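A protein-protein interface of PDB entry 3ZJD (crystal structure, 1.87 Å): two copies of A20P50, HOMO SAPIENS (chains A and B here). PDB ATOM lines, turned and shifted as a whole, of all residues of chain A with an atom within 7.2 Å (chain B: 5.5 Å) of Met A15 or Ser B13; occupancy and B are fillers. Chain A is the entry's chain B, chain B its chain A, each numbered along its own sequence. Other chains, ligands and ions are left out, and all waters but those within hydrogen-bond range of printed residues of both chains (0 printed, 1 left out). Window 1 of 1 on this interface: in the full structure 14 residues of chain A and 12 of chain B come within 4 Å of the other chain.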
ATOM      1  N   LEU A  10      -5.453  -4.118   7.848  1.00  0.00           N
ATOM      2  CA  LEU A  10      -4.006  -3.912   7.654  1.00  0.00           C
ATOM      3  C   LEU A  10      -3.354  -5.113   6.931  1.00  0.00           C
ATOM      4  O   LEU A  10      -2.610  -4.935   5.962  1.00  0.00           O
ATOM      5  CB  LEU A  10      -3.292  -3.647   8.950  1.00  0.00           C
ATOM      6  CG  LEU A  10      -2.661  -2.277   9.272  1.00  0.00           C
ATOM      7  CD1 LEU A  10      -3.446  -1.103   8.714  1.00  0.00           C
ATOM      8  CD2 LEU A  10      -2.397  -2.142  10.812  1.00  0.00           C
ATOM      9  N   TYR A  11      -3.693  -6.324   7.380  1.00  0.00           N
ATOM     10  CA  TYR A  11      -3.228  -7.589   6.794  1.00  0.00           C
ATOM     11  C   TYR A  11      -3.385  -7.686   5.282  1.00  0.00           C
ATOM     12  O   TYR A  11      -2.630  -8.405   4.606  1.00  0.00           O
ATOM     13  CB  TYR A  11      -3.990  -8.756   7.428  1.00  0.00           C
ATOM     14  N   LEU A  12      -4.375  -6.978   4.742  1.00  0.00           N
ATOM     15  CA  LEU A  12      -4.818  -7.226   3.357  1.00  0.00           C
ATOM     16  C   LEU A  12      -3.951  -6.532   2.311  1.00  0.00           C
ATOM     17  O   LEU A  12      -4.068  -6.776   1.098  1.00  0.00           O
ATOM     18  CB  LEU A  12      -6.235  -6.720   3.177  1.00  0.00           C
ATOM     19  CG  LEU A  12      -7.391  -7.563   3.648  1.00  0.00           C
ATOM     20  CD1 LEU A  12      -8.203  -7.924   2.366  1.00  0.00           C
ATOM     21  CD2 LEU A  12      -6.832  -8.759   4.318  1.00  0.00           C
ATOM     22  N   SER A  13      -3.100  -5.648   2.805  1.00  0.00           N
ATOM     23  CA  SER A  13      -2.117  -4.966   2.001  1.00  0.00           C
ATOM     24  C   SER A  13      -1.100  -5.975   1.510  1.00  0.00           C
ATOM     25  O   SER A  13      -0.402  -5.709   0.564  1.00  0.00           O
ATOM     26  CB  SER A  13      -1.438  -3.837   2.828  1.00  0.00           C
ATOM     27  OG  SER A  13      -0.708  -4.340   3.954  1.00  0.00           O
ATOM     28  N   ASN A  14      -1.009  -7.135   2.175  1.00  0.00           N
ATOM     29  CA  ASN A  14      -0.032  -8.158   1.809  1.00  0.00           C
ATOM     30  C   ASN A  14      -0.445  -9.458   2.445  1.00  0.00           C
ATOM     31  O   ASN A  14       0.033  -9.802   3.549  1.00  0.00           O
ATOM     32  CB  ASN A  14       1.374  -7.758   2.244  1.00  0.00           C
ATOM     33  CG  ASN A  14       2.431  -8.668   1.739  1.00  0.00           C
ATOM     34  OD1 ASN A  14       2.160  -9.769   1.257  1.00  0.00           O
ATOM     35  ND2 ASN A  14       3.672  -8.213   1.823  1.00  0.00           N
ATOM     36  N   MET A  15      -1.377 -10.150   1.787  1.00  0.00           N
ATOM     37  CA  MET A  15      -1.861 -11.437   2.263  1.00  0.00           C
ATOM     38  C   MET A  15      -0.745 -12.473   2.360  1.00  0.00           C
ATOM     39  O   MET A  15      -0.726 -13.275   3.289  1.00  0.00           O
ATOM     40  CB  MET A  15      -2.992 -11.969   1.387  1.00  0.00           C
ATOM     41  CG  MET A  15      -4.246 -11.091   1.387  1.00  0.00           C
ATOM     42  SD  MET A  15      -5.600 -11.892   0.519  1.00  0.00           S
ATOM     43  CE  MET A  15      -5.985 -13.211   1.679  1.00  0.00           C
ATOM     44  N   ARG A  16       0.186 -12.475   1.407  1.00  0.00           N
ATOM     45  CA  ARG A  16       1.300 -13.414   1.498  1.00  0.00           C
ATOM     46  C   ARG A  16       2.059 -13.243   2.823  1.00  0.00           C
ATOM     47  O   ARG A  16       2.340 -14.206   3.505  1.00  0.00           O
ATOM     48  CB  ARG A  16       2.273 -13.271   0.335  1.00  0.00           C
ATOM     49  CG  ARG A  16       3.481 -14.130   0.525  1.00  0.00           C
ATOM     50  CD  ARG A  16       3.006 -15.560   0.452  1.00  0.00           C
ATOM     51  NE  ARG A  16       4.057 -16.548   0.606  1.00  0.00           N
ATOM     52  CZ  ARG A  16       4.477 -17.018   1.777  1.00  0.00           C
ATOM     53  NH1 ARG A  16       3.968 -16.531   2.918  1.00  0.00           N
ATOM     54  NH2 ARG A  16       5.431 -17.942   1.797  1.00  0.00           N
ATOM     55  N   LYS A  17       2.380 -12.006   3.179  1.00  0.00           N
ATOM     56  CA  LYS A  17       3.150 -11.736   4.382  1.00  0.00           C
ATOM     57  C   LYS A  17       2.316 -12.058   5.645  1.00  0.00           C
ATOM     58  O   LYS A  17       2.831 -12.519   6.674  1.00  0.00           O
ATOM     59  CB  LYS A  17       3.611 -10.271   4.381  1.00  0.00           C
ATOM     60  CG  LYS A  17       4.096  -9.784   5.752  1.00  0.00           C
ATOM     61  CD  LYS A  17       4.497  -8.311   5.698  1.00  0.00           C
ATOM     62  CE  LYS A  17       5.649  -8.107   4.731  1.00  0.00           C
ATOM     63  NZ  LYS A  17       6.006  -6.665   4.702  1.00  0.00           N
ATOM     64  N   ALA A  18       1.023 -11.822   5.570  1.00  0.00           N
ATOM     65  CA  ALA A  18       0.165 -12.216   6.665  1.00  0.00           C
ATOM     66  C   ALA A  18       0.297 -13.694   7.007  1.00  0.00           C
ATOM     67  O   ALA A  18       0.392 -14.058   8.183  1.00  0.00           O
ATOM     68  CB  ALA A  18      -1.292 -11.840   6.390  1.00  0.00           C
ATOM     69  N   VAL A  19       0.291 -14.547   5.988  1.00  0.00           N
ATOM     70  CA  VAL A  19       0.363 -15.973   6.205  1.00  0.00           C
ATOM     71  C   VAL A  19       1.692 -16.306   6.830  1.00  0.00           C
ATOM     72  O   VAL A  19       1.790 -17.186   7.671  1.00  0.00           O
ATOM     73  CB  VAL A  19       0.215 -16.720   4.861  1.00  0.00           C
ATOM     74  CG1 VAL A  19       0.797 -18.154   4.924  1.00  0.00           C
ATOM     75  CG2 VAL A  19      -1.227 -16.733   4.453  1.00  0.00           C
ATOM     76  N   LYS A  20       2.720 -15.583   6.414  1.00  0.00           N
ATOM     77  CA  LYS A  20       4.062 -15.849   6.871  1.00  0.00           C
ATOM     78  C   LYS A  20       4.041 -15.503   8.377  1.00  0.00           C
ATOM     79  O   LYS A  20       4.572 -16.242   9.196  1.00  0.00           O
ATOM     80  CB  LYS A  20       5.037 -14.965   6.098  1.00  0.00           C
ATOM     81  CG  LYS A  20       6.444 -14.856   6.641  1.00  0.00           C
ATOM     82  CD  LYS A  20       7.409 -14.497   5.506  1.00  0.00           C
ATOM     83  CE  LYS A  20       8.281 -13.286   5.831  1.00  0.00           C
ATOM     84  NZ  LYS A  20       7.511 -11.997   5.697  1.00  0.00           N
ATOM     85  N   ILE A  21       3.369 -14.415   8.719  1.00  0.00           N
ATOM     86  CA  ILE A  21       3.296 -14.025  10.142  1.00  0.00           C
ATOM     87  C   ILE A  21       2.579 -15.085  10.965  1.00  0.00           C
ATOM     88  O   ILE A  21       3.121 -15.600  11.942  1.00  0.00           O
ATOM     89  CB  ILE A  21       2.586 -12.665  10.393  1.00  0.00           C
ATOM     90  CG1 ILE A  21       3.318 -11.526   9.691  1.00  0.00           C
ATOM     91  CG2 ILE A  21       2.561 -12.398  11.914  1.00  0.00           C
ATOM     92  CD1 ILE A  21       2.595 -10.204   9.642  1.00  0.00           C
ATOM     93  N   ARG A  22       1.367 -15.435  10.553  1.00  0.00           N
ATOM     94  CA  ARG A  22       0.649 -16.464  11.279  1.00  0.00           C
ATOM     95  C   ARG A  22       1.517 -17.724  11.341  1.00  0.00           C
ATOM     96  O   ARG A  22       1.635 -18.287  12.420  1.00  0.00           O
ATOM     97  CB  ARG A  22      -0.745 -16.723  10.702  1.00  0.00           C
ATOM     98  CG  ARG A  22      -1.787 -15.650  11.097  1.00  0.00           C
ATOM     99  CD  ARG A  22      -3.186 -15.997  10.596  1.00  0.00           C
ATOM    100  NE  ARG A  22      -3.460 -15.496   9.244  1.00  0.00           N
ATOM    101  CZ  ARG A  22      -3.453 -16.243   8.138  1.00  0.00           C
ATOM    102  NH1 ARG A  22      -3.181 -17.549   8.195  1.00  0.00           N
ATOM    103  NH2 ARG A  22      -3.716 -15.688   6.959  1.00  0.00           N
ATOM    104  N   LEU A 341       2.985  -5.380   8.741  1.00  0.00           N
ATOM    105  CA  LEU A 341       1.984  -5.155   7.719  1.00  0.00           C
ATOM    106  C   LEU A 341       1.688  -3.671   7.469  1.00  0.00           C
ATOM    107  O   LEU A 341       1.382  -3.263   6.371  1.00  0.00           O
ATOM    108  CB  LEU A 341       0.686  -5.868   8.142  1.00  0.00           C
ATOM    109  CG  LEU A 341       0.258  -7.179   7.432  1.00  0.00           C
ATOM    110  CD1 LEU A 341       1.145  -7.598   6.257  1.00  0.00           C
ATOM    111  CD2 LEU A 341       0.044  -8.379   8.363  1.00  0.00           C
ATOM    112  N   VAL B   5     -12.244 -17.958   1.815  1.00  0.00           N
ATOM    113  CA  VAL B   5     -10.921 -18.481   2.160  1.00  0.00           C
ATOM    114  C   VAL B   5      -9.847 -17.866   1.256  1.00  0.00           C
ATOM    115  O   VAL B   5      -9.330 -16.803   1.590  1.00  0.00           O
ATOM    116  CB  VAL B   5     -10.861 -20.035   2.125  1.00  0.00           C
ATOM    117  N   PRO B   7      -8.092 -15.818  -1.967  1.00  0.00           N
ATOM    118  CA  PRO B   7      -8.602 -14.553  -2.509  1.00  0.00           C
ATOM    119  C   PRO B   7      -9.479 -14.862  -3.704  1.00  0.00           C
ATOM    120  O   PRO B   7      -9.434 -15.997  -4.180  1.00  0.00           O
ATOM    121  CB  PRO B   7      -7.335 -13.777  -2.901  1.00  0.00           C
ATOM    122  CG  PRO B   7      -6.233 -14.745  -2.870  1.00  0.00           C
ATOM    123  CD  PRO B   7      -6.619 -15.867  -1.961  1.00  0.00           C
ATOM    124  N   ALA B   9      -9.533 -12.905  -6.377  1.00  0.00           N
ATOM    125  CA  ALA B   9      -8.915 -12.345  -7.553  1.00  0.00           C
ATOM    126  C   ALA B   9      -7.410 -12.323  -7.367  1.00  0.00           C
ATOM    127  O   ALA B   9      -6.935 -12.163  -6.253  1.00  0.00           O
ATOM    128  CB  ALA B   9      -9.442 -10.950  -7.807  1.00  0.00           C
ATOM    129  N   LEU B  10      -6.646 -12.447  -8.458  1.00  0.00           N
ATOM    130  CA  LEU B  10      -5.210 -12.598  -8.299  1.00  0.00           C
ATOM    131  C   LEU B  10      -4.582 -11.485  -7.510  1.00  0.00           C
ATOM    132  O   LEU B  10      -3.852 -11.749  -6.565  1.00  0.00           O
ATOM    133  CB  LEU B  10      -4.537 -12.744  -9.652  1.00  0.00           C
ATOM    134  CG  LEU B  10      -3.030 -12.851  -9.717  1.00  0.00           C
ATOM    135  CD1 LEU B  10      -2.578 -14.121  -9.089  1.00  0.00           C
ATOM    136  CD2 LEU B  10      -2.638 -12.836 -11.249  1.00  0.00           C
ATOM    137  N   TYR B  11      -4.882 -10.234  -7.873  1.00  0.00           N
ATOM    138  CA  TYR B  11      -4.188  -9.072  -7.291  1.00  0.00           C
ATOM    139  C   TYR B  11      -4.330  -8.974  -5.771  1.00  0.00           C
ATOM    140  O   TYR B  11      -3.568  -8.295  -5.105  1.00  0.00           O
ATOM    141  CB  TYR B  11      -4.580  -7.740  -7.984  1.00  0.00           C
ATOM    142  CG  TYR B  11      -5.949  -7.204  -7.611  1.00  0.00           C
ATOM    143  CD1 TYR B  11      -7.112  -7.905  -7.929  1.00  0.00           C
ATOM    144  CD2 TYR B  11      -6.081  -5.996  -6.931  1.00  0.00           C
ATOM    145  CE1 TYR B  11      -8.383  -7.410  -7.583  1.00  0.00           C
ATOM    146  CE2 TYR B  11      -7.333  -5.491  -6.584  1.00  0.00           C
ATOM    147  CZ  TYR B  11      -8.483  -6.199  -6.909  1.00  0.00           C
ATOM    148  OH  TYR B  11      -9.720  -5.689  -6.547  1.00  0.00           O
ATOM    149  N   LEU B  12      -5.299  -9.664  -5.205  1.00  0.00           N
ATOM    150  CA  LEU B  12      -5.445  -9.589  -3.771  1.00  0.00           C
ATOM    151  C   LEU B  12      -4.306 -10.287  -3.012  1.00  0.00           C
ATOM    152  O   LEU B  12      -4.328 -10.292  -1.795  1.00  0.00           O
ATOM    153  CB  LEU B  12      -6.785 -10.204  -3.337  1.00  0.00           C
ATOM    154  CG  LEU B  12      -8.072  -9.384  -3.206  1.00  0.00           C
ATOM    155  CD1 LEU B  12      -8.283  -8.504  -4.390  1.00  0.00           C
ATOM    156  CD2 LEU B  12      -9.270 -10.323  -3.053  1.00  0.00           C
ATOM    157  N   SER B  13      -3.333 -10.895  -3.696  1.00  0.00           N
ATOM    158  CA  SER B  13      -2.440 -11.831  -2.983  1.00  0.00           C
ATOM    159  C   SER B  13      -1.257 -11.124  -2.303  1.00  0.00           C
ATOM    160  O   SER B  13      -0.704 -11.602  -1.300  1.00  0.00           O
ATOM    161  CB  SER B  13      -1.927 -12.938  -3.913  1.00  0.00           C
ATOM    162  OG  SER B  13      -0.848 -12.468  -4.718  1.00  0.00           O
ATOM    163  N   ASN B  14      -0.849 -10.012  -2.900  1.00  0.00           N
ATOM    164  CA  ASN B  14       0.190  -9.176  -2.354  1.00  0.00           C
ATOM    165  C   ASN B  14       0.052  -7.796  -2.964  1.00  0.00           C
ATOM    166  O   ASN B  14       0.749  -7.488  -3.933  1.00  0.00           O
ATOM    167  CB  ASN B  14       1.558  -9.768  -2.650  1.00  0.00           C
ATOM    168  CG  ASN B  14       2.646  -9.103  -1.869  1.00  0.00           C
ATOM    169  OD1 ASN B  14       2.492  -7.959  -1.393  1.00  0.00           O
ATOM    170  ND2 ASN B  14       3.767  -9.795  -1.730  1.00  0.00           N
ATOM    171  N   MET B  15      -0.870  -6.990  -2.430  1.00  0.00           N
ATOM    172  CA  MET B  15      -1.155  -5.667  -3.020  1.00  0.00           C
ATOM    173  C   MET B  15       0.060  -4.739  -2.950  1.00  0.00           C
ATOM    174  O   MET B  15       0.287  -3.942  -3.852  1.00  0.00           O
ATOM    175  CB  MET B  15      -2.410  -5.013  -2.428  1.00  0.00           C
ATOM    176  CG  MET B  15      -3.719  -5.823  -2.530  1.00  0.00           C
ATOM    177  SD  MET B  15      -5.138  -4.938  -1.796  1.00  0.00           S
ATOM    178  CE  MET B  15      -5.248  -3.581  -2.992  1.00  0.00           C
ATOM    179  N   LEU B 341       2.905 -12.001  -8.603  1.00  0.00           N
ATOM    180  CA  LEU B 341       1.725 -12.240  -7.807  1.00  0.00           C
ATOM    181  C   LEU B 341       1.367 -13.700  -7.864  1.00  0.00           C
ATOM    182  O   LEU B 341       0.786 -14.206  -6.943  1.00  0.00           O
ATOM    183  CB  LEU B 341       0.549 -11.408  -8.306  1.00  0.00           C
ATOM    184  CG  LEU B 341       0.626  -9.911  -7.941  1.00  0.00           C
ATOM    185  CD1 LEU B 341      -0.784  -9.256  -8.115  1.00  0.00           C
ATOM    186  CD2 LEU B 341       1.208  -9.703  -6.537  1.00  0.00           C
ATOM    187  N   VAL B 342       1.682 -14.390  -8.972  1.00  0.00           N
ATOM    188  CA  VAL B 342       1.146 -15.729  -9.078  1.00  0.00           C
ATOM    189  C   VAL B 342       1.875 -16.656  -8.129  1.00  0.00           C
ATOM    190  O   VAL B 342       1.280 -17.564  -7.513  1.00  0.00           O
ATOM    191  CB  VAL B 342       1.149 -16.252 -10.562  1.00  0.00           C
ATOM    192  CG1 VAL B 342       0.927 -17.733 -10.578  1.00  0.00           C
ATOM    193  CG2 VAL B 342       0.050 -15.527 -11.403  1.00  0.00           C
ATOM    194  N   ASP B 344       3.070 -15.700  -5.226  1.00  0.00           N
ATOM    195  CA  ASP B 344       2.578 -15.391  -3.884  1.00  0.00           C
ATOM    196  C   ASP B 344       1.213 -16.028  -3.721  1.00  0.00           C
ATOM    197  O   ASP B 344       0.853 -16.524  -2.648  1.00  0.00           O
ATOM    198  CB  ASP B 344       2.524 -13.877  -3.681  1.00  0.00           C
ATOM    199  CG  ASP B 344       3.874 -13.304  -3.274  1.00  0.00           C
ATOM    200  OD1 ASP B 344       4.732 -14.077  -2.770  1.00  0.00           O
ATOM    201  OD2 ASP B 344       4.084 -12.084  -3.449  1.00  0.00           O
ATOM    202  N   TYR B 345       0.489 -16.086  -4.825  1.00  0.00           N
ATOM    203  CA  TYR B 345      -0.857 -16.636  -4.848  1.00  0.00           C
ATOM    204  C   TYR B 345      -0.768 -18.127  -4.543  1.00  0.00           C
ATOM    205  O   TYR B 345      -1.499 -18.657  -3.711  1.00  0.00           O
ATOM    206  CB  TYR B 345      -1.513 -16.417  -6.234  1.00  0.00           C
ATOM    207  CG  TYR B 345      -2.988 -16.656  -6.159  1.00  0.00           C
ATOM    208  CD1 TYR B 345      -3.507 -17.949  -6.169  1.00  0.00           C
ATOM    209  CD2 TYR B 345      -3.857 -15.605  -6.011  1.00  0.00           C
ATOM    210  CE1 TYR B 345      -4.835 -18.171  -6.083  1.00  0.00           C
ATOM    211  CE2 TYR B 345      -5.201 -15.826  -5.869  1.00  0.00           C
ATOM    212  CZ  TYR B 345      -5.689 -17.111  -5.905  1.00  0.00           C
ATOM    213  OH  TYR B 345      -7.030 -17.326  -5.777  1.00  0.00           O
ATOM    214  N   LEU B 348      -0.129 -18.939  -1.018  1.00  0.00           N
ATOM    215  CA  LEU B 348      -1.393 -18.803  -0.295  1.00  0.00           C
ATOM    216  C   LEU B 348      -2.285 -20.029  -0.470  1.00  0.00           C
ATOM    217  O   LEU B 348      -2.942 -20.459   0.489  1.00  0.00           O
ATOM    218  CB  LEU B 348      -2.155 -17.572  -0.764  1.00  0.00           C
ATOM    219  CG  LEU B 348      -2.438 -16.385   0.135  1.00  0.00           C
ATOM    220  CD1 LEU B 348      -1.260 -16.073   1.037  1.00  0.00           C
ATOM    221  CD2 LEU B 348      -2.765 -15.194  -0.690  1.00  0.00           C
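O of Ser B13 is in hydrogen-bond range of N of Met A15 (3.5 Å). O of Ser B13 is in hydrogen-bond range of N of Arg A16 (3.0 Å). The side-chain amide oxygen of Asn B14 lies close to the side-chain amide oxygen of Asn A14 (3.2 Å). The backbone NH (N) of Met B15 sits at hydrogen-bond distance from the backbone carbonyl oxygen (O) of Ser A13, 3.3 Å away. The backbone carbonyl oxygen (O) of Leu A12 lies close to the side-chain sulfur (SD) of Met B15, 3.6 Å away. O of Leu B12 lies close to SD of Met A15.
OG of Ser B13 is in hydrogen-bond range of O of Leu B341 (3.3 Å). ND2 of Asn B14 lies within hydrogen-bond range of OD2 of Asp B344 (2.9 Å). O of Leu A10 is in hydrogen-bond range of OG of Ser A13 (2.8 Å). O of Leu A341 sits at hydrogen-bond distance from OG of Ser A13. OD1 of Asn A14 lies close to N of Arg A16, at 3.4 Å. The side-chain amide oxygen (OD1) of Asn A14 lies within hydrogen-bond range of the backbone NH (N) of Lys A17, at 3.0 Å.
O of Met A15 touches CD1 of Leu B348, at 3.6 Å. Arg A16 touches Asp B344. Leu B348 touches Arg A16. Leu B348 touches Val A19 (CD1 to CG2, 3.5 Å).
Met A15 touches just these residues of chain B: Leu B12 (3.1 Å), Ser B13 (3.5 Å) and Leu B348 (3.6 Å). Ser B13 touches just these residues of chain A: Met A15 and Arg A16. Printed residues of chain A within 4 Å of Leu B348: Met A15 (3.6 Å), Arg A16 (3.7 Å) and Val A19 (3.5 Å). Of the printed residues of chain B, Leu A12 touches Met B15. Printed residues of chain A within 4 Å of Leu B12: Met A15 (3.1 Å). Leu B341 touches none of the printed residues of chain A. Lys A20 touches none of the printed residues of chain B. The nearest printed residue of chain B that does not touch Val A19 is Asp B344 (7.4 Å).
Hydrophobic or aromatic side chains of chain A within 4 Å of the printed part of chain B: Met A15 and Val A19. Printed residues of chain B that touch a printed residue of chain A: Leu B12, Ser B13, Asn B14, Met B15, Asp B344 and Leu B348. Hydrophobic or aromatic side chains of chain B that line the printed part of chain A: Met B15 and Leu B348. Along chain B the printed residues that touch a printed residue of chain A span positions 12 to 348. Among the printed residues, 10 pairs touch across the chains. Among the printed residues, no Asp or Glu carboxylate lies within 4 Å of a Lys or Arg side-chain nitrogen of the other chain.
Leu A12 touches Met B15, and with the chains exchanged Met A15 touches Leu B12. Ser A13 touches Met B15, and with the chains exchanged Met A15 touches Ser B13. Asn A14 touches its own counterpart, Asn B14.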
